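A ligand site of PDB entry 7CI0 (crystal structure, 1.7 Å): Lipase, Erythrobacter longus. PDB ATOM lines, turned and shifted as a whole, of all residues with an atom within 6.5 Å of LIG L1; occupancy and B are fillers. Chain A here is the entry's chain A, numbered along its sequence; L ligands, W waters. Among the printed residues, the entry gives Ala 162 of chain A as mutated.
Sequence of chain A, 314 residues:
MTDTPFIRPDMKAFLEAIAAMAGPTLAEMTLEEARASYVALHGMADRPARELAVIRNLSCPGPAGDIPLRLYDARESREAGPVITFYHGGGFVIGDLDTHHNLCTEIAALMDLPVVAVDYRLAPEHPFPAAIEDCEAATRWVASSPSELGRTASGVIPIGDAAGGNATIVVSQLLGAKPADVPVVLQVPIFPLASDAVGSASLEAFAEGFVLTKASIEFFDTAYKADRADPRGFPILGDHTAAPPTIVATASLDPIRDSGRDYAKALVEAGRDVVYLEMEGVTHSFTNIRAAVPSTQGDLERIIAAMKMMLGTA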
ATOM      1  N   GLY A  89      36.630 -23.151  24.248  1.00  0.00           N
ATOM      2  CA  GLY A  89      35.263 -22.958  23.812  1.00  0.00           C
ATOM      3  C   GLY A  89      35.191 -22.562  22.348  1.00  0.00           C
ATOM      4  O   GLY A  89      36.200 -22.496  21.647  1.00  0.00           O
ATOM      5  N   GLY A  90      33.974 -22.292  21.895  1.00  0.00           N
ATOM      6  CA  GLY A  90      33.762 -22.097  20.471  1.00  0.00           C
ATOM      7  C   GLY A  90      32.702 -22.982  19.864  1.00  0.00           C
ATOM      8  O   GLY A  90      32.697 -23.229  18.649  1.00  0.00           O
ATOM      9  N   GLY A  91      31.769 -23.455  20.690  1.00  0.00           N
ATOM     10  CA  GLY A  91      30.616 -24.163  20.170  1.00  0.00           C
ATOM     11  C   GLY A  91      30.902 -25.532  19.597  1.00  0.00           C
ATOM     12  O   GLY A  91      30.010 -26.131  19.001  1.00  0.00           O
ATOM     13  N   PHE A  92      32.118 -26.030  19.794  1.00  0.00           N
ATOM     14  CA  PHE A  92      32.654 -27.225  19.147  1.00  0.00           C
ATOM     15  C   PHE A  92      32.814 -27.039  17.645  1.00  0.00           C
ATOM     16  O   PHE A  92      32.990 -28.020  16.910  1.00  0.00           O
ATOM     17  CB  PHE A  92      31.789 -28.453  19.455  1.00  0.00           C
ATOM     18  CG  PHE A  92      31.748 -28.823  20.922  1.00  0.00           C
ATOM     19  CD1 PHE A  92      32.926 -29.112  21.602  1.00  0.00           C
ATOM     20  CD2 PHE A  92      30.555 -28.902  21.614  1.00  0.00           C
ATOM     21  CE1 PHE A  92      32.918 -29.471  22.947  1.00  0.00           C
ATOM     22  CE2 PHE A  92      30.533 -29.250  22.963  1.00  0.00           C
ATOM     23  CZ  PHE A  92      31.715 -29.539  23.626  1.00  0.00           C
ATOM     24  N   ALA A 162      32.709 -22.451  28.079  1.00  0.00           N
ATOM     25  CA  ALA A 162      31.545 -22.640  27.206  1.00  0.00           C
ATOM     26  C   ALA A 162      31.518 -24.083  26.702  1.00  0.00           C
ATOM     27  O   ALA A 162      31.318 -24.923  27.505  1.00  0.00           O
ATOM     28  CB  ALA A 162      31.573 -21.625  26.090  1.00  0.00           C
ATOM     29  N   ALA A 163      31.719 -24.316  25.417  1.00  0.00           N
ATOM     30  CA  ALA A 163      31.772 -25.708  24.926  1.00  0.00           C
ATOM     31  C   ALA A 163      32.868 -26.447  25.709  1.00  0.00           C
ATOM     32  O   ALA A 163      32.669 -27.584  26.027  1.00  0.00           O
ATOM     33  CB  ALA A 163      32.042 -25.722  23.457  1.00  0.00           C
ATOM     34  N   PHE A 191      31.444 -20.778  32.410  1.00  0.00           N
ATOM     35  CA  PHE A 191      30.223 -20.482  31.615  1.00  0.00           C
ATOM     36  C   PHE A 191      29.860 -21.697  30.756  1.00  0.00           C
ATOM     37  O   PHE A 191      29.762 -21.594  29.563  1.00  0.00           O
ATOM     38  CB  PHE A 191      30.228 -19.111  30.930  1.00  0.00           C
ATOM     39  CG  PHE A 191      31.510 -18.637  30.311  1.00  0.00           C
ATOM     40  CD1 PHE A 191      31.884 -19.048  29.062  1.00  0.00           C
ATOM     41  CD2 PHE A 191      32.303 -17.728  30.960  1.00  0.00           C
ATOM     42  CE1 PHE A 191      33.052 -18.585  28.489  1.00  0.00           C
ATOM     43  CE2 PHE A 191      33.486 -17.282  30.407  1.00  0.00           C
ATOM     44  CZ  PHE A 191      33.847 -17.712  29.166  1.00  0.00           C
ATOM     45  N   PRO A 192      29.638 -22.862  31.357  1.00  0.00           N
ATOM     46  CA  PRO A 192      29.397 -24.055  30.607  1.00  0.00           C
ATOM     47  C   PRO A 192      27.974 -24.251  30.124  1.00  0.00           C
ATOM     48  O   PRO A 192      27.111 -23.694  30.592  1.00  0.00           O
ATOM     49  CB  PRO A 192      29.586 -25.142  31.662  1.00  0.00           C
ATOM     50  CG  PRO A 192      29.086 -24.506  32.911  1.00  0.00           C
ATOM     51  CD  PRO A 192      29.587 -23.085  32.790  1.00  0.00           C
ATOM     52  N   LEU A 193      27.896 -25.078  29.105  1.00  0.00           N
ATOM     53  CA  LEU A 193      26.606 -25.610  28.674  1.00  0.00           C
ATOM     54  C   LEU A 193      26.429 -26.968  29.349  1.00  0.00           C
ATOM     55  O   LEU A 193      27.140 -27.925  29.018  1.00  0.00           O
ATOM     56  CB  LEU A 193      26.557 -25.739  27.151  1.00  0.00           C
ATOM     57  CG  LEU A 193      25.171 -25.969  26.520  1.00  0.00           C
ATOM     58  CD1 LEU A 193      24.644 -27.360  26.809  1.00  0.00           C
ATOM     59  CD2 LEU A 193      24.177 -24.903  26.977  1.00  0.00           C
ATOM     60  N   SER A 195      22.803 -27.942  30.950  1.00  0.00           N
ATOM     61  CA  SER A 195      21.437 -28.193  30.498  1.00  0.00           C
ATOM     62  C   SER A 195      21.192 -27.414  29.206  1.00  0.00           C
ATOM     63  O   SER A 195      21.803 -26.375  28.977  1.00  0.00           O
ATOM     64  CB  SER A 195      20.425 -27.760  31.555  1.00  0.00           C
ATOM     65  OG  SER A 195      20.539 -26.377  31.849  1.00  0.00           O
ATOM     66  N   ASP A 196      20.285 -27.938  28.381  1.00  0.00           N
ATOM     67  CA  ASP A 196      19.854 -27.256  27.163  1.00  0.00           C
ATOM     68  C   ASP A 196      19.455 -25.818  27.440  1.00  0.00           C
ATOM     69  O   ASP A 196      18.604 -25.547  28.294  1.00  0.00           O
ATOM     70  CB  ASP A 196      18.685 -28.053  26.563  1.00  0.00           C
ATOM     71  CG  ASP A 196      18.351 -27.646  25.141  1.00  0.00           C
ATOM     72  OD1 ASP A 196      18.918 -26.671  24.615  1.00  0.00           O
ATOM     73  OD2 ASP A 196      17.494 -28.338  24.546  1.00  0.00           O
ATOM     74  N   ALA A 197      20.055 -24.871  26.713  1.00  0.00           N
ATOM     75  CA  ALA A 197      19.724 -23.462  26.912  1.00  0.00           C
ATOM     76  C   ALA A 197      18.411 -23.086  26.258  1.00  0.00           C
ATOM     77  O   ALA A 197      17.792 -22.088  26.645  1.00  0.00           O
ATOM     78  CB  ALA A 197      20.857 -22.584  26.359  1.00  0.00           C
ATOM     79  N   VAL A 198      17.963 -23.867  25.273  1.00  0.00           N
ATOM     80  CA  VAL A 198      16.696 -23.557  24.618  1.00  0.00           C
ATOM     81  C   VAL A 198      15.581 -23.583  25.648  1.00  0.00           C
ATOM     82  O   VAL A 198      15.445 -24.534  26.428  1.00  0.00           O
ATOM     83  CB  VAL A 198      16.458 -24.549  23.474  1.00  0.00           C
ATOM     84  CG1 VAL A 198      15.107 -24.270  22.811  1.00  0.00           C
ATOM     85  CG2 VAL A 198      17.586 -24.436  22.464  1.00  0.00           C
ATOM     86  N   LEU A 212      27.947 -13.687  22.930  1.00  0.00           N
ATOM     87  CA  LEU A 212      27.362 -14.956  22.454  1.00  0.00           C
ATOM     88  C   LEU A 212      25.893 -14.686  22.132  1.00  0.00           C
ATOM     89  O   LEU A 212      25.200 -14.267  22.993  1.00  0.00           O
ATOM     90  CB  LEU A 212      27.476 -16.048  23.517  1.00  0.00           C
ATOM     91  CG  LEU A 212      26.923 -17.395  23.101  1.00  0.00           C
ATOM     92  CD1 LEU A 212      27.678 -17.908  21.899  1.00  0.00           C
ATOM     93  CD2 LEU A 212      26.953 -18.404  24.223  1.00  0.00           C
ATOM     94  N   SER A 216      24.279 -17.552  17.073  1.00  0.00           N
ATOM     95  CA  SER A 216      25.471 -18.391  17.101  1.00  0.00           C
ATOM     96  C   SER A 216      25.176 -19.732  17.759  1.00  0.00           C
ATOM     97  O   SER A 216      25.662 -20.772  17.301  1.00  0.00           O
ATOM     98  CB  SER A 216      26.616 -17.662  17.798  1.00  0.00           C
ATOM     99  OG  SER A 216      27.006 -16.505  17.078  1.00  0.00           O
ATOM    100  N   ILE A 217      24.400 -19.725  18.848  1.00  0.00           N
ATOM    101  CA  ILE A 217      24.018 -20.985  19.505  1.00  0.00           C
ATOM    102  C   ILE A 217      23.322 -21.916  18.520  1.00  0.00           C
ATOM    103  O   ILE A 217      23.621 -23.117  18.462  1.00  0.00           O
ATOM    104  CB  ILE A 217      23.135 -20.691  20.738  1.00  0.00           C
ATOM    105  CG1 ILE A 217      23.977 -20.068  21.851  1.00  0.00           C
ATOM    106  CG2 ILE A 217      22.442 -21.976  21.200  1.00  0.00           C
ATOM    107  CD1 ILE A 217      23.155 -19.392  22.985  1.00  0.00           C
ATOM    108  N   GLU A 218      22.404 -21.376  17.719  1.00  0.00           N
ATOM    109  CA  GLU A 218      21.698 -22.219  16.756  1.00  0.00           C
ATOM    110  C   GLU A 218      22.629 -22.713  15.649  1.00  0.00           C
ATOM    111  O   GLU A 218      22.513 -23.864  15.204  1.00  0.00           O
ATOM    112  CB  GLU A 218      20.507 -21.445  16.198  1.00  0.00           C
ATOM    113  CG  GLU A 218      19.459 -21.182  17.272  1.00  0.00           C
ATOM    114  CD  GLU A 218      18.342 -20.260  16.816  1.00  0.00           C
ATOM    115  OE1 GLU A 218      18.528 -19.533  15.820  1.00  0.00           O
ATOM    116  OE2 GLU A 218      17.275 -20.257  17.468  1.00  0.00           O
ATOM    117  N   PHE A 220      25.842 -23.313  16.060  1.00  0.00           N
ATOM    118  CA  PHE A 220      26.614 -24.366  16.698  1.00  0.00           C
ATOM    119  C   PHE A 220      25.807 -25.650  16.837  1.00  0.00           C
ATOM    120  O   PHE A 220      26.324 -26.743  16.582  1.00  0.00           O
ATOM    121  CB  PHE A 220      27.081 -23.898  18.085  1.00  0.00           C
ATOM    122  CG  PHE A 220      28.097 -22.786  18.066  1.00  0.00           C
ATOM    123  CD1 PHE A 220      29.067 -22.715  17.081  1.00  0.00           C
ATOM    124  CD2 PHE A 220      28.084 -21.804  19.059  1.00  0.00           C
ATOM    125  CE1 PHE A 220      30.029 -21.705  17.092  1.00  0.00           C
ATOM    126  CE2 PHE A 220      29.033 -20.783  19.074  1.00  0.00           C
ATOM    127  CZ  PHE A 220      30.003 -20.734  18.099  1.00  0.00           C
ATOM    128  N   ASP A 221      24.544 -25.538  17.273  1.00  0.00           N
ATOM    129  CA  ASP A 221      23.685 -26.721  17.402  1.00  0.00           C
ATOM    130  C   ASP A 221      23.615 -27.488  16.093  1.00  0.00           C
ATOM    131  O   ASP A 221      23.781 -28.714  16.055  1.00  0.00           O
ATOM    132  CB  ASP A 221      22.275 -26.309  17.827  1.00  0.00           C
ATOM    133  CG  ASP A 221      22.144 -26.042  19.317  1.00  0.00           C
ATOM    134  OD1 ASP A 221      23.138 -26.209  20.044  1.00  0.00           O
ATOM    135  OD2 ASP A 221      21.032 -25.681  19.747  1.00  0.00           O
ATOM    136  N   ARG A 228      19.671 -34.302  22.215  1.00  0.00           N
ATOM    137  CA  ARG A 228      19.244 -33.700  23.472  1.00  0.00           C
ATOM    138  C   ARG A 228      19.077 -34.713  24.589  1.00  0.00           C
ATOM    139  O   ARG A 228      19.036 -34.326  25.762  1.00  0.00           O
ATOM    140  CB  ARG A 228      17.935 -32.928  23.262  1.00  0.00           C
ATOM    141  CG  ARG A 228      18.054 -31.426  23.305  1.00  0.00           C
ATOM    142  CD  ARG A 228      18.783 -30.842  22.121  1.00  0.00           C
ATOM    143  NE  ARG A 228      18.884 -29.390  22.287  1.00  0.00           N
ATOM    144  CZ  ARG A 228      19.587 -28.587  21.494  1.00  0.00           C
ATOM    145  NH1 ARG A 228      20.234 -29.084  20.449  1.00  0.00           N
ATOM    146  NH2 ARG A 228      19.615 -27.281  21.743  1.00  0.00           N
ATOM    147  N   PHE A 234      24.520 -33.188  26.861  1.00  0.00           N
ATOM    148  CA  PHE A 234      23.853 -32.367  27.864  1.00  0.00           C
ATOM    149  C   PHE A 234      24.090 -33.020  29.210  1.00  0.00           C
ATOM    150  O   PHE A 234      23.269 -33.824  29.695  1.00  0.00           O
ATOM    151  CB  PHE A 234      22.367 -32.208  27.521  1.00  0.00           C
ATOM    152  CG  PHE A 234      22.167 -31.534  26.195  1.00  0.00           C
ATOM    153  CD1 PHE A 234      22.172 -32.280  25.016  1.00  0.00           C
ATOM    154  CD2 PHE A 234      22.083 -30.151  26.107  1.00  0.00           C
ATOM    155  CE1 PHE A 234      22.036 -31.642  23.778  1.00  0.00           C
ATOM    156  CE2 PHE A 234      21.939 -29.516  24.873  1.00  0.00           C
ATOM    157  CZ  PHE A 234      21.923 -30.269  23.718  1.00  0.00           C
ATOM    158  N   ILE A 256      23.518 -18.406  28.238  1.00  0.00           N
ATOM    159  CA  ILE A 256      23.531 -19.757  28.804  1.00  0.00           C
ATOM    160  C   ILE A 256      23.859 -19.730  30.300  1.00  0.00           C
ATOM    161  O   ILE A 256      24.193 -20.754  30.886  1.00  0.00           O
ATOM    162  CB  ILE A 256      24.476 -20.694  28.038  1.00  0.00           C
ATOM    163  CG1 ILE A 256      25.953 -20.337  28.235  1.00  0.00           C
ATOM    164  CG2 ILE A 256      24.124 -20.692  26.539  1.00  0.00           C
ATOM    165  CD1 ILE A 256      26.892 -21.439  27.682  1.00  0.00           C
ATOM    166  N   HIS A 284      29.283 -13.728  28.675  1.00  0.00           N
ATOM    167  CA  HIS A 284      29.982 -14.850  28.060  1.00  0.00           C
ATOM    168  C   HIS A 284      31.312 -14.366  27.504  1.00  0.00           C
ATOM    169  O   HIS A 284      31.417 -13.212  27.044  1.00  0.00           O
ATOM    170  CB  HIS A 284      29.104 -15.427  26.954  1.00  0.00           C
ATOM    171  CG  HIS A 284      29.504 -16.805  26.499  1.00  0.00           C
ATOM    172  ND1 HIS A 284      29.073 -17.948  27.142  1.00  0.00           N
ATOM    173  CD2 HIS A 284      30.289 -17.215  25.469  1.00  0.00           C
ATOM    174  CE1 HIS A 284      29.564 -19.017  26.517  1.00  0.00           C
ATOM    175  NE2 HIS A 284      30.312 -18.590  25.504  1.00  0.00           N
HETATM  176  C1  LIG L   1      26.782 -23.208  23.026  1.00  0.00           C
HETATM  177  C2  LIG L   1      25.733 -23.172  23.997  1.00  0.00           C
HETATM  178  C3  LIG L   1      24.525 -23.807  23.765  1.00  0.00           C
HETATM  179  C4  LIG L   1      24.339 -24.472  22.588  1.00  0.00           C
HETATM  180  C5  LIG L   1      25.383 -24.510  21.604  1.00  0.00           C
HETATM  181  C6  LIG L   1      26.588 -23.883  21.846  1.00  0.00           C
HETATM  182  O1  LIG L   1      23.125 -25.109  22.343  1.00  0.00           O
HETATM  183  N1  LIG L   1      28.060 -22.547  23.303  1.00  0.00           N
HETATM  184  O2  LIG L   1      29.079 -22.473  22.328  1.00  0.00           O
HETATM  185  O3  LIG L   1      28.264 -22.049  24.415  1.00  0.00           O
HETATM  186  C1  LG2 L   2      27.249 -27.343  22.710  1.00  0.00           C
HETATM  187  C2  LG2 L   2      27.025 -27.211  21.362  1.00  0.00           C
HETATM  188  C3  LG2 L   2      26.019 -27.949  20.811  1.00  0.00           C
HETATM  189  C4  LG2 L   2      25.279 -28.789  21.570  1.00  0.00           C
HETATM  190  C5  LG2 L   2      25.488 -28.919  22.884  1.00  0.00           C
HETATM  191  C6  LG2 L   2      26.481 -28.193  23.450  1.00  0.00           C
HETATM  192  O1  LG2 L   2      24.322 -29.502  21.018  1.00  0.00           O
HETATM  193  N1  LG2 L   2      28.216 -26.611  23.347  1.00  0.00           N
HETATM  194  O2  LG2 L   2      28.831 -25.620  22.738  1.00  0.00           O
HETATM  195  O3  LG2 L   2      28.479 -26.784  24.446  1.00  0.00           O
HETATM  196  C1  LG3 L   3      31.462 -16.253  20.290  1.00  0.00           C
HETATM  197  C2  LG3 L   3      31.085 -16.514  19.011  1.00  0.00           C
HETATM  198  C3  LG3 L   3      31.052 -15.451  18.152  1.00  0.00           C
HETATM  199  C4  LG3 L   3      31.347 -14.190  18.569  1.00  0.00           C
HETATM  200  C5  LG3 L   3      31.688 -13.964  19.844  1.00  0.00           C
HETATM  201  C6  LG3 L   3      31.756 -14.999  20.701  1.00  0.00           C
HETATM  202  O1  LG3 L   3      31.291 -13.142  17.775  1.00  0.00           O
HETATM  203  N1  LG3 L   3      31.575 -17.279  21.151  1.00  0.00           N
HETATM  204  O2  LG3 L   3      31.333 -18.536  20.727  1.00  0.00           O
HETATM  205  O3  LG3 L   3      32.004 -17.091  22.235  1.00  0.00           O
HETATM  206  O   HOH W   1      21.538 -25.777  24.417  1.00  0.00           O
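Water W1 lies within hydrogen-bond range of an oxygen (O1) of LIG L1 (2.7 Å), the side-chain carboxylate (OD1) of Asp 196 (2.8 Å) and the backbone NH (N) of Ala 197 (2.9 Å).
CB of Ala 162 touches O3 of LIG L1 (3.7 Å).
Leu 193 touches LIG L1.
CD2 of Leu 212 touches O3 of LIG L1 (3.9 Å).
Ile 217 touches LIG L1 (CG2 to O1, 3.4 Å).
CD2 of Phe 220 touches O2 of LIG L1, at 3.5 Å.
Ile 256 touches LIG L1 (CD1 to O3, 3.6 Å).
His 284 touches LIG L1.
Hydrophobic or aromatic side chains within 4 Å of LIG L1: Ala 162, Leu 193, Leu 212, Ile 217, Phe 220, Ile 256 and His 284.
An oxygen (O1) of LIG L1 lies within hydrogen-bond range of the side-chain carboxylate (OD1) of Asp 221 (2.5 Å).
O2 of LIG L1 sits close to N of Gly 91 (3.3 Å).
The side-chain carboxylate of Asp 221 is in salt-bridge range of the guanidinium group of Arg 228 (2.9 Å).
The backbone NH of Ala 162 lies close to the backbone carbonyl oxygen of Phe 191.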
